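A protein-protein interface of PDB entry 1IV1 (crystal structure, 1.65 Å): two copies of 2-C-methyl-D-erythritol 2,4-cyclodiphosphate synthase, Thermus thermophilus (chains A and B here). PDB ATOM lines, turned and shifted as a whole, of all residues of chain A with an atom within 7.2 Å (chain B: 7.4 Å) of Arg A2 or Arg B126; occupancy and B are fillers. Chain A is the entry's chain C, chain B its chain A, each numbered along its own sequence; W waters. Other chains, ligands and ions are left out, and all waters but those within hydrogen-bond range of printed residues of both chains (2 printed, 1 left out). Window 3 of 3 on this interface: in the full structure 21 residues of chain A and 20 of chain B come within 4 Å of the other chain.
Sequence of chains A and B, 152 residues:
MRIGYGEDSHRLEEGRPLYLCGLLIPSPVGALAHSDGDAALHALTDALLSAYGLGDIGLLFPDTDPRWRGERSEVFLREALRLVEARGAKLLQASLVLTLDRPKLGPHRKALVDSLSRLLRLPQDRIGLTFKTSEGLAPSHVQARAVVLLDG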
ATOM      1  N   ARG A   2      30.206  23.372 -25.015  1.00  0.00           N
ATOM      2  CA  ARG A   2      29.051  22.925 -24.246  1.00  0.00           C
ATOM      3  C   ARG A   2      29.142  21.435 -23.906  1.00  0.00           C
ATOM      4  O   ARG A   2      29.496  20.602 -24.742  1.00  0.00           O
ATOM      5  CB  ARG A   2      27.739  23.146 -24.996  1.00  0.00           C
ATOM      6  CG  ARG A   2      27.367  24.600 -25.268  1.00  0.00           C
ATOM      7  CD  ARG A   2      25.858  24.745 -25.365  1.00  0.00           C
ATOM      8  NE  ARG A   2      25.401  26.117 -25.556  1.00  0.00           N
ATOM      9  CZ  ARG A   2      24.633  26.750 -24.676  1.00  0.00           C
ATOM     10  NH1 ARG A   2      24.244  26.143 -23.563  1.00  0.00           N
ATOM     11  NH2 ARG A   2      24.254  27.999 -24.919  1.00  0.00           N
ATOM     12  N   ILE A   3      28.790  21.167 -22.661  1.00  0.00           N
ATOM     13  CA  ILE A   3      28.757  19.825 -22.094  1.00  0.00           C
ATOM     14  C   ILE A   3      27.373  19.513 -21.545  1.00  0.00           C
ATOM     15  O   ILE A   3      26.578  20.347 -21.107  1.00  0.00           O
ATOM     16  CB  ILE A   3      29.865  19.687 -21.030  1.00  0.00           C
ATOM     17  CG1 ILE A   3      30.082  18.246 -20.562  1.00  0.00           C
ATOM     18  CG2 ILE A   3      29.622  20.620 -19.844  1.00  0.00           C
ATOM     19  CD1 ILE A   3      31.305  18.047 -19.707  1.00  0.00           C
ATOM     20  N   GLY A   4      27.020  18.229 -21.564  1.00  0.00           N
ATOM     21  CA  GLY A   4      25.733  17.787 -21.056  1.00  0.00           C
ATOM     22  C   GLY A   4      25.901  16.373 -20.505  1.00  0.00           C
ATOM     23  O   GLY A   4      26.683  15.588 -21.026  1.00  0.00           O
ATOM     24  N   SER A  50      20.078  18.702 -21.916  1.00  0.00           N
ATOM     25  CA  SER A  50      20.711  19.277 -20.733  1.00  0.00           C
ATOM     26  C   SER A  50      21.767  20.299 -21.140  1.00  0.00           C
ATOM     27  O   SER A  50      22.027  21.325 -20.494  1.00  0.00           O
ATOM     28  CB  SER A  50      21.332  18.171 -19.880  1.00  0.00           C
ATOM     29  OG  SER A  50      21.878  18.640 -18.668  1.00  0.00           O
ATOM     30  N   ALA A  51      22.404  20.030 -22.286  1.00  0.00           N
ATOM     31  CA  ALA A  51      23.472  20.923 -22.715  1.00  0.00           C
ATOM     32  C   ALA A  51      22.940  22.321 -23.038  1.00  0.00           C
ATOM     33  O   ALA A  51      23.776  23.220 -23.124  1.00  0.00           O
ATOM     34  CB  ALA A  51      24.203  20.390 -23.939  1.00  0.00           C
ATOM     35  N   TYR A  52      21.632  22.438 -23.230  1.00  0.00           N
ATOM     36  CA  TYR A  52      21.021  23.699 -23.646  1.00  0.00           C
ATOM     37  C   TYR A  52      19.908  24.109 -22.706  1.00  0.00           C
ATOM     38  O   TYR A  52      19.128  25.004 -23.013  1.00  0.00           O
ATOM     39  CB  TYR A  52      20.498  23.583 -25.087  1.00  0.00           C
ATOM     40  CG  TYR A  52      21.606  23.913 -26.055  1.00  0.00           C
ATOM     41  CD1 TYR A  52      22.510  22.911 -26.404  1.00  0.00           C
ATOM     42  CD2 TYR A  52      21.770  25.178 -26.599  1.00  0.00           C
ATOM     43  CE1 TYR A  52      23.535  23.207 -27.285  1.00  0.00           C
ATOM     44  CE2 TYR A  52      22.804  25.462 -27.485  1.00  0.00           C
ATOM     45  CZ  TYR A  52      23.688  24.458 -27.828  1.00  0.00           C
ATOM     46  OH  TYR A  52      24.737  24.683 -28.699  1.00  0.00           O
ATOM     47  N   GLY A  53      19.851  23.436 -21.575  1.00  0.00           N
ATOM     48  CA  GLY A  53      18.843  23.570 -20.560  1.00  0.00           C
ATOM     49  C   GLY A  53      17.420  23.413 -21.057  1.00  0.00           C
ATOM     50  O   GLY A  53      16.516  24.030 -20.483  1.00  0.00           O
ATOM     51  N   ARG A  87      19.576  25.669 -32.142  1.00  0.00           N
ATOM     52  CA  ARG A  87      20.176  26.624 -31.215  1.00  0.00           C
ATOM     53  C   ARG A  87      21.658  26.858 -31.518  1.00  0.00           C
ATOM     54  O   ARG A  87      22.378  27.516 -30.758  1.00  0.00           O
ATOM     55  CB  ARG A  87      19.924  26.123 -29.787  1.00  0.00           C
ATOM     56  CG  ARG A  87      18.568  26.630 -29.267  1.00  0.00           C
ATOM     57  CD  ARG A  87      17.834  25.493 -28.595  1.00  0.00           C
ATOM     58  NE  ARG A  87      16.431  25.751 -28.301  1.00  0.00           N
ATOM     59  CZ  ARG A  87      15.421  25.394 -29.085  1.00  0.00           C
ATOM     60  NH1 ARG A  87      15.639  24.763 -30.233  1.00  0.00           N
ATOM     61  NH2 ARG A  87      14.185  25.683 -28.703  1.00  0.00           N
ATOM     62  N   ALA A  89      23.885  24.295 -32.047  1.00  0.00           N
ATOM     63  CA  ALA A  89      24.921  23.363 -31.578  1.00  0.00           C
ATOM     64  C   ALA A  89      25.485  22.505 -32.696  1.00  0.00           C
ATOM     65  O   ALA A  89      24.898  22.233 -33.744  1.00  0.00           O
ATOM     66  CB  ALA A  89      24.354  22.520 -30.447  1.00  0.00           C
ATOM     67  N   LYS A  90      26.714  22.042 -32.489  1.00  0.00           N
ATOM     68  CA  LYS A  90      27.308  21.007 -33.331  1.00  0.00           C
ATOM     69  C   LYS A  90      27.873  19.925 -32.414  1.00  0.00           C
ATOM     70  O   LYS A  90      28.828  20.115 -31.678  1.00  0.00           O
ATOM     71  CB  LYS A  90      28.371  21.563 -34.276  1.00  0.00           C
ATOM     72  CG  LYS A  90      27.769  22.721 -35.065  1.00  0.00           C
ATOM     73  CD  LYS A  90      28.774  23.770 -35.506  1.00  0.00           C
ATOM     74  CE  LYS A  90      28.025  24.748 -36.418  1.00  0.00           C
ATOM     75  NZ  LYS A  90      26.557  24.568 -36.220  1.00  0.00           N
ATOM     76  N   LEU A  92      29.881  17.078 -31.064  1.00  0.00           N
ATOM     77  CA  LEU A  92      31.258  16.698 -31.313  1.00  0.00           C
ATOM     78  C   LEU A  92      31.556  15.309 -30.787  1.00  0.00           C
ATOM     79  O   LEU A  92      32.366  14.538 -31.302  1.00  0.00           O
ATOM     80  CB  LEU A  92      32.166  17.747 -30.645  1.00  0.00           C
ATOM     81  CG  LEU A  92      33.662  17.585 -30.890  1.00  0.00           C
ATOM     82  CD1 LEU A  92      33.987  17.958 -32.334  1.00  0.00           C
ATOM     83  CD2 LEU A  92      34.477  18.426 -29.926  1.00  0.00           C
ATOM     84  N   GLN A  93      30.938  14.938 -29.673  1.00  0.00           N
ATOM     85  CA  GLN A  93      31.337  13.686 -29.055  1.00  0.00           C
ATOM     86  C   GLN A  93      30.310  13.209 -28.042  1.00  0.00           C
ATOM     87  O   GLN A  93      29.659  13.978 -27.340  1.00  0.00           O
ATOM     88  CB  GLN A  93      32.716  13.835 -28.398  1.00  0.00           C
ATOM     89  CG  GLN A  93      33.213  12.541 -27.778  1.00  0.00           C
ATOM     90  CD  GLN A  93      34.694  12.512 -27.464  1.00  0.00           C
ATOM     91  OE1 GLN A  93      35.307  11.442 -27.425  1.00  0.00           O
ATOM     92  NE2 GLN A  93      35.278  13.679 -27.242  1.00  0.00           N
ATOM     93  N   VAL A 148      27.978  14.343 -23.239  1.00  0.00           N
ATOM     94  CA  VAL A 148      28.042  14.831 -24.601  1.00  0.00           C
ATOM     95  C   VAL A 148      28.907  16.115 -24.561  1.00  0.00           C
ATOM     96  O   VAL A 148      28.882  16.802 -23.546  1.00  0.00           O
ATOM     97  CB  VAL A 148      26.690  15.127 -25.275  1.00  0.00           C
ATOM     98  CG1 VAL A 148      25.920  13.834 -25.576  1.00  0.00           C
ATOM     99  CG2 VAL A 148      25.797  16.062 -24.465  1.00  0.00           C
ATOM    100  N   LEU A 149      29.619  16.360 -25.636  1.00  0.00           N
ATOM    101  CA  LEU A 149      30.399  17.576 -25.850  1.00  0.00           C
ATOM    102  C   LEU A 149      29.946  18.219 -27.153  1.00  0.00           C
ATOM    103  O   LEU A 149      29.809  17.498 -28.153  1.00  0.00           O
ATOM    104  CB  LEU A 149      31.882  17.217 -25.900  1.00  0.00           C
ATOM    105  CG  LEU A 149      32.876  18.367 -26.048  1.00  0.00           C
ATOM    106  CD1 LEU A 149      32.789  19.288 -24.838  1.00  0.00           C
ATOM    107  CD2 LEU A 149      34.288  17.840 -26.245  1.00  0.00           C
ATOM    108  N   LEU A 150      29.704  19.523 -27.204  1.00  0.00           N
ATOM    109  CA  LEU A 150      29.269  20.167 -28.442  1.00  0.00           C
ATOM    110  C   LEU A 150      30.075  21.446 -28.688  1.00  0.00           C
ATOM    111  O   LEU A 150      30.460  22.090 -27.715  1.00  0.00           O
ATOM    112  CB  LEU A 150      27.786  20.537 -28.454  1.00  0.00           C
ATOM    113  CG  LEU A 150      26.867  19.358 -28.065  1.00  0.00           C
ATOM    114  CD1 LEU A 150      26.640  19.325 -26.561  1.00  0.00           C
ATOM    115  CD2 LEU A 150      25.560  19.402 -28.838  1.00  0.00           C
ATOM    116  N   ASP A 151      30.256  21.702 -29.964  1.00  0.00           N
ATOM    117  CA  ASP A 151      30.912  22.872 -30.519  1.00  0.00           C
ATOM    118  C   ASP A 151      32.435  22.774 -30.446  1.00  0.00           C
ATOM    119  O   ASP A 151      33.097  22.676 -31.485  1.00  0.00           O
ATOM    120  CB  ASP A 151      30.405  24.119 -29.789  1.00  0.00           C
ATOM    121  CG  ASP A 151      28.925  24.354 -30.014  1.00  0.00           C
ATOM    122  OD1 ASP A 151      28.324  23.601 -30.814  1.00  0.00           O
ATOM    123  OD2 ASP A 151      28.369  25.279 -29.383  1.00  0.00           O
ATOM    124  N   LEU B  91      33.107  29.900 -13.933  1.00  0.00           N
ATOM    125  CA  LEU B  91      32.160  28.798 -14.190  1.00  0.00           C
ATOM    126  C   LEU B  91      31.361  29.106 -15.446  1.00  0.00           C
ATOM    127  O   LEU B  91      30.824  30.195 -15.636  1.00  0.00           O
ATOM    128  CB  LEU B  91      31.238  28.552 -13.012  1.00  0.00           C
ATOM    129  CG  LEU B  91      30.077  27.567 -13.149  1.00  0.00           C
ATOM    130  CD1 LEU B  91      30.583  26.170 -13.487  1.00  0.00           C
ATOM    131  CD2 LEU B  91      29.262  27.516 -11.862  1.00  0.00           C
ATOM    132  N   LEU B  92      31.286  28.095 -16.312  1.00  0.00           N
ATOM    133  CA  LEU B  92      30.619  28.300 -17.599  1.00  0.00           C
ATOM    134  C   LEU B  92      29.349  27.473 -17.716  1.00  0.00           C
ATOM    135  O   LEU B  92      28.362  27.900 -18.308  1.00  0.00           O
ATOM    136  CB  LEU B  92      31.658  27.971 -18.652  1.00  0.00           C
ATOM    137  CG  LEU B  92      31.295  27.646 -20.084  1.00  0.00           C
ATOM    138  CD1 LEU B  92      30.388  28.689 -20.700  1.00  0.00           C
ATOM    139  CD2 LEU B  92      32.595  27.524 -20.887  1.00  0.00           C
ATOM    140  N   GLN B  93      29.328  26.261 -17.150  1.00  0.00           N
ATOM    141  CA  GLN B  93      28.149  25.424 -17.327  1.00  0.00           C
ATOM    142  C   GLN B  93      28.071  24.401 -16.204  1.00  0.00           C
ATOM    143  O   GLN B  93      29.066  23.964 -15.625  1.00  0.00           O
ATOM    144  CB  GLN B  93      28.183  24.725 -18.691  1.00  0.00           C
ATOM    145  CG  GLN B  93      26.931  23.923 -19.016  1.00  0.00           C
ATOM    146  CD  GLN B  93      26.745  23.657 -20.499  1.00  0.00           C
ATOM    147  OE1 GLN B  93      25.631  23.589 -21.031  1.00  0.00           O
ATOM    148  NE2 GLN B  93      27.846  23.497 -21.213  1.00  0.00           N
ATOM    149  N   ALA B  94      26.833  24.026 -15.892  1.00  0.00           N
ATOM    150  CA  ALA B  94      26.608  22.953 -14.934  1.00  0.00           C
ATOM    151  C   ALA B  94      25.495  22.046 -15.473  1.00  0.00           C
ATOM    152  O   ALA B  94      24.406  22.499 -15.818  1.00  0.00           O
ATOM    153  CB  ALA B  94      26.269  23.482 -13.552  1.00  0.00           C
ATOM    154  N   SER B  95      25.810  20.739 -15.525  1.00  0.00           N
ATOM    155  CA  SER B  95      24.767  19.802 -15.984  1.00  0.00           C
ATOM    156  C   SER B  95      24.583  18.710 -14.947  1.00  0.00           C
ATOM    157  O   SER B  95      25.543  18.028 -14.585  1.00  0.00           O
ATOM    158  CB  SER B  95      25.195  19.280 -17.347  1.00  0.00           C
ATOM    159  OG  SER B  95      24.214  18.421 -17.919  1.00  0.00           O
ATOM    160  N   LEU B  96      23.368  18.505 -14.433  1.00  0.00           N
ATOM    161  CA  LEU B  96      23.196  17.483 -13.406  1.00  0.00           C
ATOM    162  C   LEU B  96      21.864  16.743 -13.520  1.00  0.00           C
ATOM    163  O   LEU B  96      20.882  17.231 -14.054  1.00  0.00           O
ATOM    164  CB  LEU B  96      23.300  18.080 -12.004  1.00  0.00           C
ATOM    165  CG  LEU B  96      22.250  19.121 -11.604  1.00  0.00           C
ATOM    166  CD1 LEU B  96      22.177  19.244 -10.087  1.00  0.00           C
ATOM    167  CD2 LEU B  96      22.537  20.474 -12.237  1.00  0.00           C
ATOM    168  N   VAL B 113      15.462  25.370 -11.523  1.00  0.00           N
ATOM    169  CA  VAL B 113      16.438  25.918 -12.471  1.00  0.00           C
ATOM    170  C   VAL B 113      16.737  27.385 -12.123  1.00  0.00           C
ATOM    171  O   VAL B 113      17.898  27.777 -12.139  1.00  0.00           O
ATOM    172  CB  VAL B 113      15.962  25.790 -13.922  1.00  0.00           C
ATOM    173  CG1 VAL B 113      16.870  26.551 -14.875  1.00  0.00           C
ATOM    174  CG2 VAL B 113      15.884  24.312 -14.291  1.00  0.00           C
ATOM    175  N   LEU B 120      24.465  29.817  -9.044  1.00  0.00           N
ATOM    176  CA  LEU B 120      25.709  29.593  -9.773  1.00  0.00           C
ATOM    177  C   LEU B 120      26.141  30.781 -10.640  1.00  0.00           C
ATOM    178  O   LEU B 120      27.232  30.734 -11.213  1.00  0.00           O
ATOM    179  CB  LEU B 120      25.561  28.367 -10.681  1.00  0.00           C
ATOM    180  CG  LEU B 120      25.976  27.010 -10.120  1.00  0.00           C
ATOM    181  CD1 LEU B 120      25.837  26.926  -8.620  1.00  0.00           C
ATOM    182  CD2 LEU B 120      25.165  25.900 -10.808  1.00  0.00           C
ATOM    183  N   LEU B 122      24.807  31.702 -13.546  1.00  0.00           N
ATOM    184  CA  LEU B 122      24.805  31.249 -14.920  1.00  0.00           C
ATOM    185  C   LEU B 122      23.446  31.545 -15.559  1.00  0.00           C
ATOM    186  O   LEU B 122      22.410  31.485 -14.894  1.00  0.00           O
ATOM    187  CB  LEU B 122      25.105  29.745 -15.041  1.00  0.00           C
ATOM    188  CG  LEU B 122      26.504  29.250 -14.652  1.00  0.00           C
ATOM    189  CD1 LEU B 122      26.542  27.721 -14.593  1.00  0.00           C
ATOM    190  CD2 LEU B 122      27.589  29.728 -15.601  1.00  0.00           C
ATOM    191  N   PRO B 123      23.468  31.839 -16.852  1.00  0.00           N
ATOM    192  CA  PRO B 123      22.235  31.980 -17.638  1.00  0.00           C
ATOM    193  C   PRO B 123      21.497  30.643 -17.680  1.00  0.00           C
ATOM    194  O   PRO B 123      22.137  29.612 -17.469  1.00  0.00           O
ATOM    195  CB  PRO B 123      22.738  32.371 -19.022  1.00  0.00           C
ATOM    196  CG  PRO B 123      24.169  31.984 -19.071  1.00  0.00           C
ATOM    197  CD  PRO B 123      24.681  32.042 -17.663  1.00  0.00           C
ATOM    198  N   GLN B 124      20.203  30.614 -17.920  1.00  0.00           N
ATOM    199  CA  GLN B 124      19.372  29.434 -17.807  1.00  0.00           C
ATOM    200  C   GLN B 124      19.745  28.326 -18.787  1.00  0.00           C
ATOM    201  O   GLN B 124      19.539  27.139 -18.507  1.00  0.00           O
ATOM    202  CB  GLN B 124      17.901  29.793 -18.072  1.00  0.00           C
ATOM    203  CG  GLN B 124      17.342  30.834 -17.122  1.00  0.00           C
ATOM    204  CD  GLN B 124      16.605  30.197 -15.961  1.00  0.00           C
ATOM    205  OE1 GLN B 124      15.498  29.688 -16.129  1.00  0.00           O
ATOM    206  NE2 GLN B 124      17.230  30.222 -14.789  1.00  0.00           N
ATOM    207  N   ASP B 125      20.258  28.738 -19.943  1.00  0.00           N
ATOM    208  CA  ASP B 125      20.621  27.772 -20.976  1.00  0.00           C
ATOM    209  C   ASP B 125      21.956  27.115 -20.678  1.00  0.00           C
ATOM    210  O   ASP B 125      22.388  26.224 -21.413  1.00  0.00           O
ATOM    211  CB  ASP B 125      20.709  28.462 -22.336  1.00  0.00           C
ATOM    212  CG  ASP B 125      21.808  29.506 -22.386  1.00  0.00           C
ATOM    213  OD1 ASP B 125      22.988  29.148 -22.541  1.00  0.00           O
ATOM    214  OD2 ASP B 125      21.483  30.708 -22.259  1.00  0.00           O
ATOM    215  N   ARG B 126      22.610  27.553 -19.617  1.00  0.00           N
ATOM    216  CA  ARG B 126      23.838  26.939 -19.130  1.00  0.00           C
ATOM    217  C   ARG B 126      23.563  26.135 -17.864  1.00  0.00           C
ATOM    218  O   ARG B 126      24.427  25.612 -17.176  1.00  0.00           O
ATOM    219  CB  ARG B 126      24.915  28.007 -18.916  1.00  0.00           C
ATOM    220  CG  ARG B 126      25.542  28.482 -20.225  1.00  0.00           C
ATOM    221  CD  ARG B 126      26.372  27.426 -20.917  1.00  0.00           C
ATOM    222  NE  ARG B 126      27.023  27.946 -22.120  1.00  0.00           N
ATOM    223  CZ  ARG B 126      28.100  27.427 -22.704  1.00  0.00           C
ATOM    224  NH1 ARG B 126      28.735  26.353 -22.254  1.00  0.00           N
ATOM    225  NH2 ARG B 126      28.588  28.006 -23.794  1.00  0.00           N
ATOM    226  N   ILE B 127      22.284  26.001 -17.500  1.00  0.00           N
ATOM    227  CA  ILE B 127      21.917  25.159 -16.376  1.00  0.00           C
ATOM    228  C   ILE B 127      21.233  23.907 -16.949  1.00  0.00           C
ATOM    229  O   ILE B 127      20.132  24.106 -17.452  1.00  0.00           O
ATOM    230  CB  ILE B 127      20.919  25.816 -15.409  1.00  0.00           C
ATOM    231  CG1 ILE B 127      21.462  27.044 -14.661  1.00  0.00           C
ATOM    232  CG2 ILE B 127      20.399  24.763 -14.457  1.00  0.00           C
ATOM    233  CD1 ILE B 127      22.815  26.785 -14.025  1.00  0.00           C
ATOM    234  N   GLY B 128      21.892  22.759 -16.872  1.00  0.00           N
ATOM    235  CA  GLY B 128      21.318  21.544 -17.441  1.00  0.00           C
ATOM    236  C   GLY B 128      20.804  20.663 -16.325  1.00  0.00           C
ATOM    237  O   GLY B 128      21.564  19.920 -15.691  1.00  0.00           O
ATOM    238  N   LEU B 129      19.511  20.756 -16.068  1.00  0.00           N
ATOM    239  CA  LEU B 129      18.879  20.005 -14.994  1.00  0.00           C
ATOM    240  C   LEU B 129      17.894  18.963 -15.533  1.00  0.00           C
ATOM    241  O   LEU B 129      16.964  19.344 -16.239  1.00  0.00           O
ATOM    242  CB  LEU B 129      18.107  20.963 -14.089  1.00  0.00           C
ATOM    243  CG  LEU B 129      17.352  20.331 -12.925  1.00  0.00           C
ATOM    244  CD1 LEU B 129      18.292  19.431 -12.127  1.00  0.00           C
ATOM    245  CD2 LEU B 129      16.734  21.401 -12.033  1.00  0.00           C
ATOM    246  N   VAL B 147      28.162  17.368 -13.587  1.00  0.00           N
ATOM    247  CA  VAL B 147      29.336  17.798 -14.326  1.00  0.00           C
ATOM    248  C   VAL B 147      29.386  19.321 -14.423  1.00  0.00           C
ATOM    249  O   VAL B 147      28.328  19.906 -14.666  1.00  0.00           O
ATOM    250  CB  VAL B 147      29.309  17.198 -15.740  1.00  0.00           C
ATOM    251  CG1 VAL B 147      30.515  17.668 -16.529  1.00  0.00           C
ATOM    252  CG2 VAL B 147      29.262  15.679 -15.630  1.00  0.00           C
ATOM    253  N   LEU B 149      31.735  22.683 -16.108  1.00  0.00           N
ATOM    254  CA  LEU B 149      32.728  23.122 -17.074  1.00  0.00           C
ATOM    255  C   LEU B 149      33.116  24.558 -16.694  1.00  0.00           C
ATOM    256  O   LEU B 149      32.194  25.321 -16.414  1.00  0.00           O
ATOM    257  CB  LEU B 149      32.154  23.052 -18.474  1.00  0.00           C
ATOM    258  CG  LEU B 149      32.949  23.547 -19.671  1.00  0.00           C
ATOM    259  CD1 LEU B 149      34.173  22.687 -19.960  1.00  0.00           C
ATOM    260  CD2 LEU B 149      32.039  23.600 -20.894  1.00  0.00           C
HETATM  261  O   HOH W   1      21.335  16.717 -16.841  1.00  0.00           O
HETATM  262  O   HOH W   2      17.201  26.476 -19.092  1.00  0.00           O
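The backbone NH of Ile A3 lies close to the side-chain amide nitrogen of Gln B93, 2.9 Å away.
OE1 of Gln B93 lies close to O of Ala A51, 2.8 Å away.
OG of Ser A50 is in hydrogen-bond range of OG of Ser B95, at 2.5 Å.
The side-chain carboxylate (OD1) of Asp B125 lies within salt-bridge range of the guanidinium group (NH2) of Arg A2 (2.9 Å).
The backbone carbonyl oxygen of Gly B128 lies close to the side-chain hydroxyl of Ser A50.
The backbone NH (N) of Leu B92 is in hydrogen-bond range of the backbone carbonyl oxygen (O) of Leu B149, at 2.9 Å.
The backbone NH (N) of Leu B149 lies within hydrogen-bond range of the backbone carbonyl oxygen (O) of Gln B93 (3.0 Å).
N of Ala B94 is in hydrogen-bond range of O of Arg B126, at 3.2 Å.
N of Gly B128 sits at hydrogen-bond distance from O of Ala B94.
The backbone NH (N) of Leu B96 sits at hydrogen-bond distance from the backbone carbonyl oxygen (O) of Gly B128, 2.6 Å away.
The backbone NH of Leu A150 sits at hydrogen-bond distance from the backbone carbonyl oxygen of Arg A2 (2.7 Å).
Gln B93 touches Arg A2 (NE2 to CA, 3.3 Å).
Arg B126 touches Arg A2.
Val B147 touches Ile A3 (CG1 to CD1, 3.3 Å).
CG2 of Ile A3 touches CB of Leu B149, 3.8 Å away.
Gly A4 touches Ser B95 (CA to OG, 3.5 Å).
Ala A51 touches Asp B125.
Asp B125 touches Tyr A52 (O to C, 3.5 Å).
N of Gly A53 touches O of Asp B125, 3.8 Å away.
Ile B127 touches Gly A53 (O to CA, 3.4 Å).
Printed residues of chain B within 4 Å of Arg A2: Gln B93, Asp B125 and Arg B126.
Arg B126 touches just one residue of chain A: Arg A2 (3.6 Å).
Printed residues of chain B within 4 Å of Gly A53: Asp B125 (3.8 Å) and Ile B127 (3.4 Å).
Printed residues of chain B within 4 Å of Gly A4: Ser B95.
Of the printed residues of chain A, Gly B128 touches Ser A50.
Of the printed residues of chain A, Gln B93 touches Arg A2 (3.3 Å), Ile A3 (2.9 Å) and Ala A51 (2.8 Å).
Of the printed residues of chain A, Ser B95 touches Gly A4 (3.5 Å) and Ser A50 (2.5 Å).
The nearest printed residue of chain B that does not touch Ala A51 is Ser B95 (5.0 Å).
Hydrophobic or aromatic side chains of chain A that line the printed part of chain B: Ile A3.
Among the printed residues, 14 pairs touch across the chains.
Positions printed for both chains: 92, 93 and 149.
Water W2 bridges the backbone carbonyl oxygen (O) of Gln B124 (2.5 Å) and the backbone carbonyl oxygen (O) of Gly A53 (2.9 Å).
Water W1 lies within hydrogen-bond range of the side-chain hydroxyl (OG) of Ser A50 (2.7 Å), the backbone carbonyl oxygen (O) of Leu B96 (2.9 Å) and the backbone carbonyl oxygen (O) of Gly B128 (3.4 Å).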
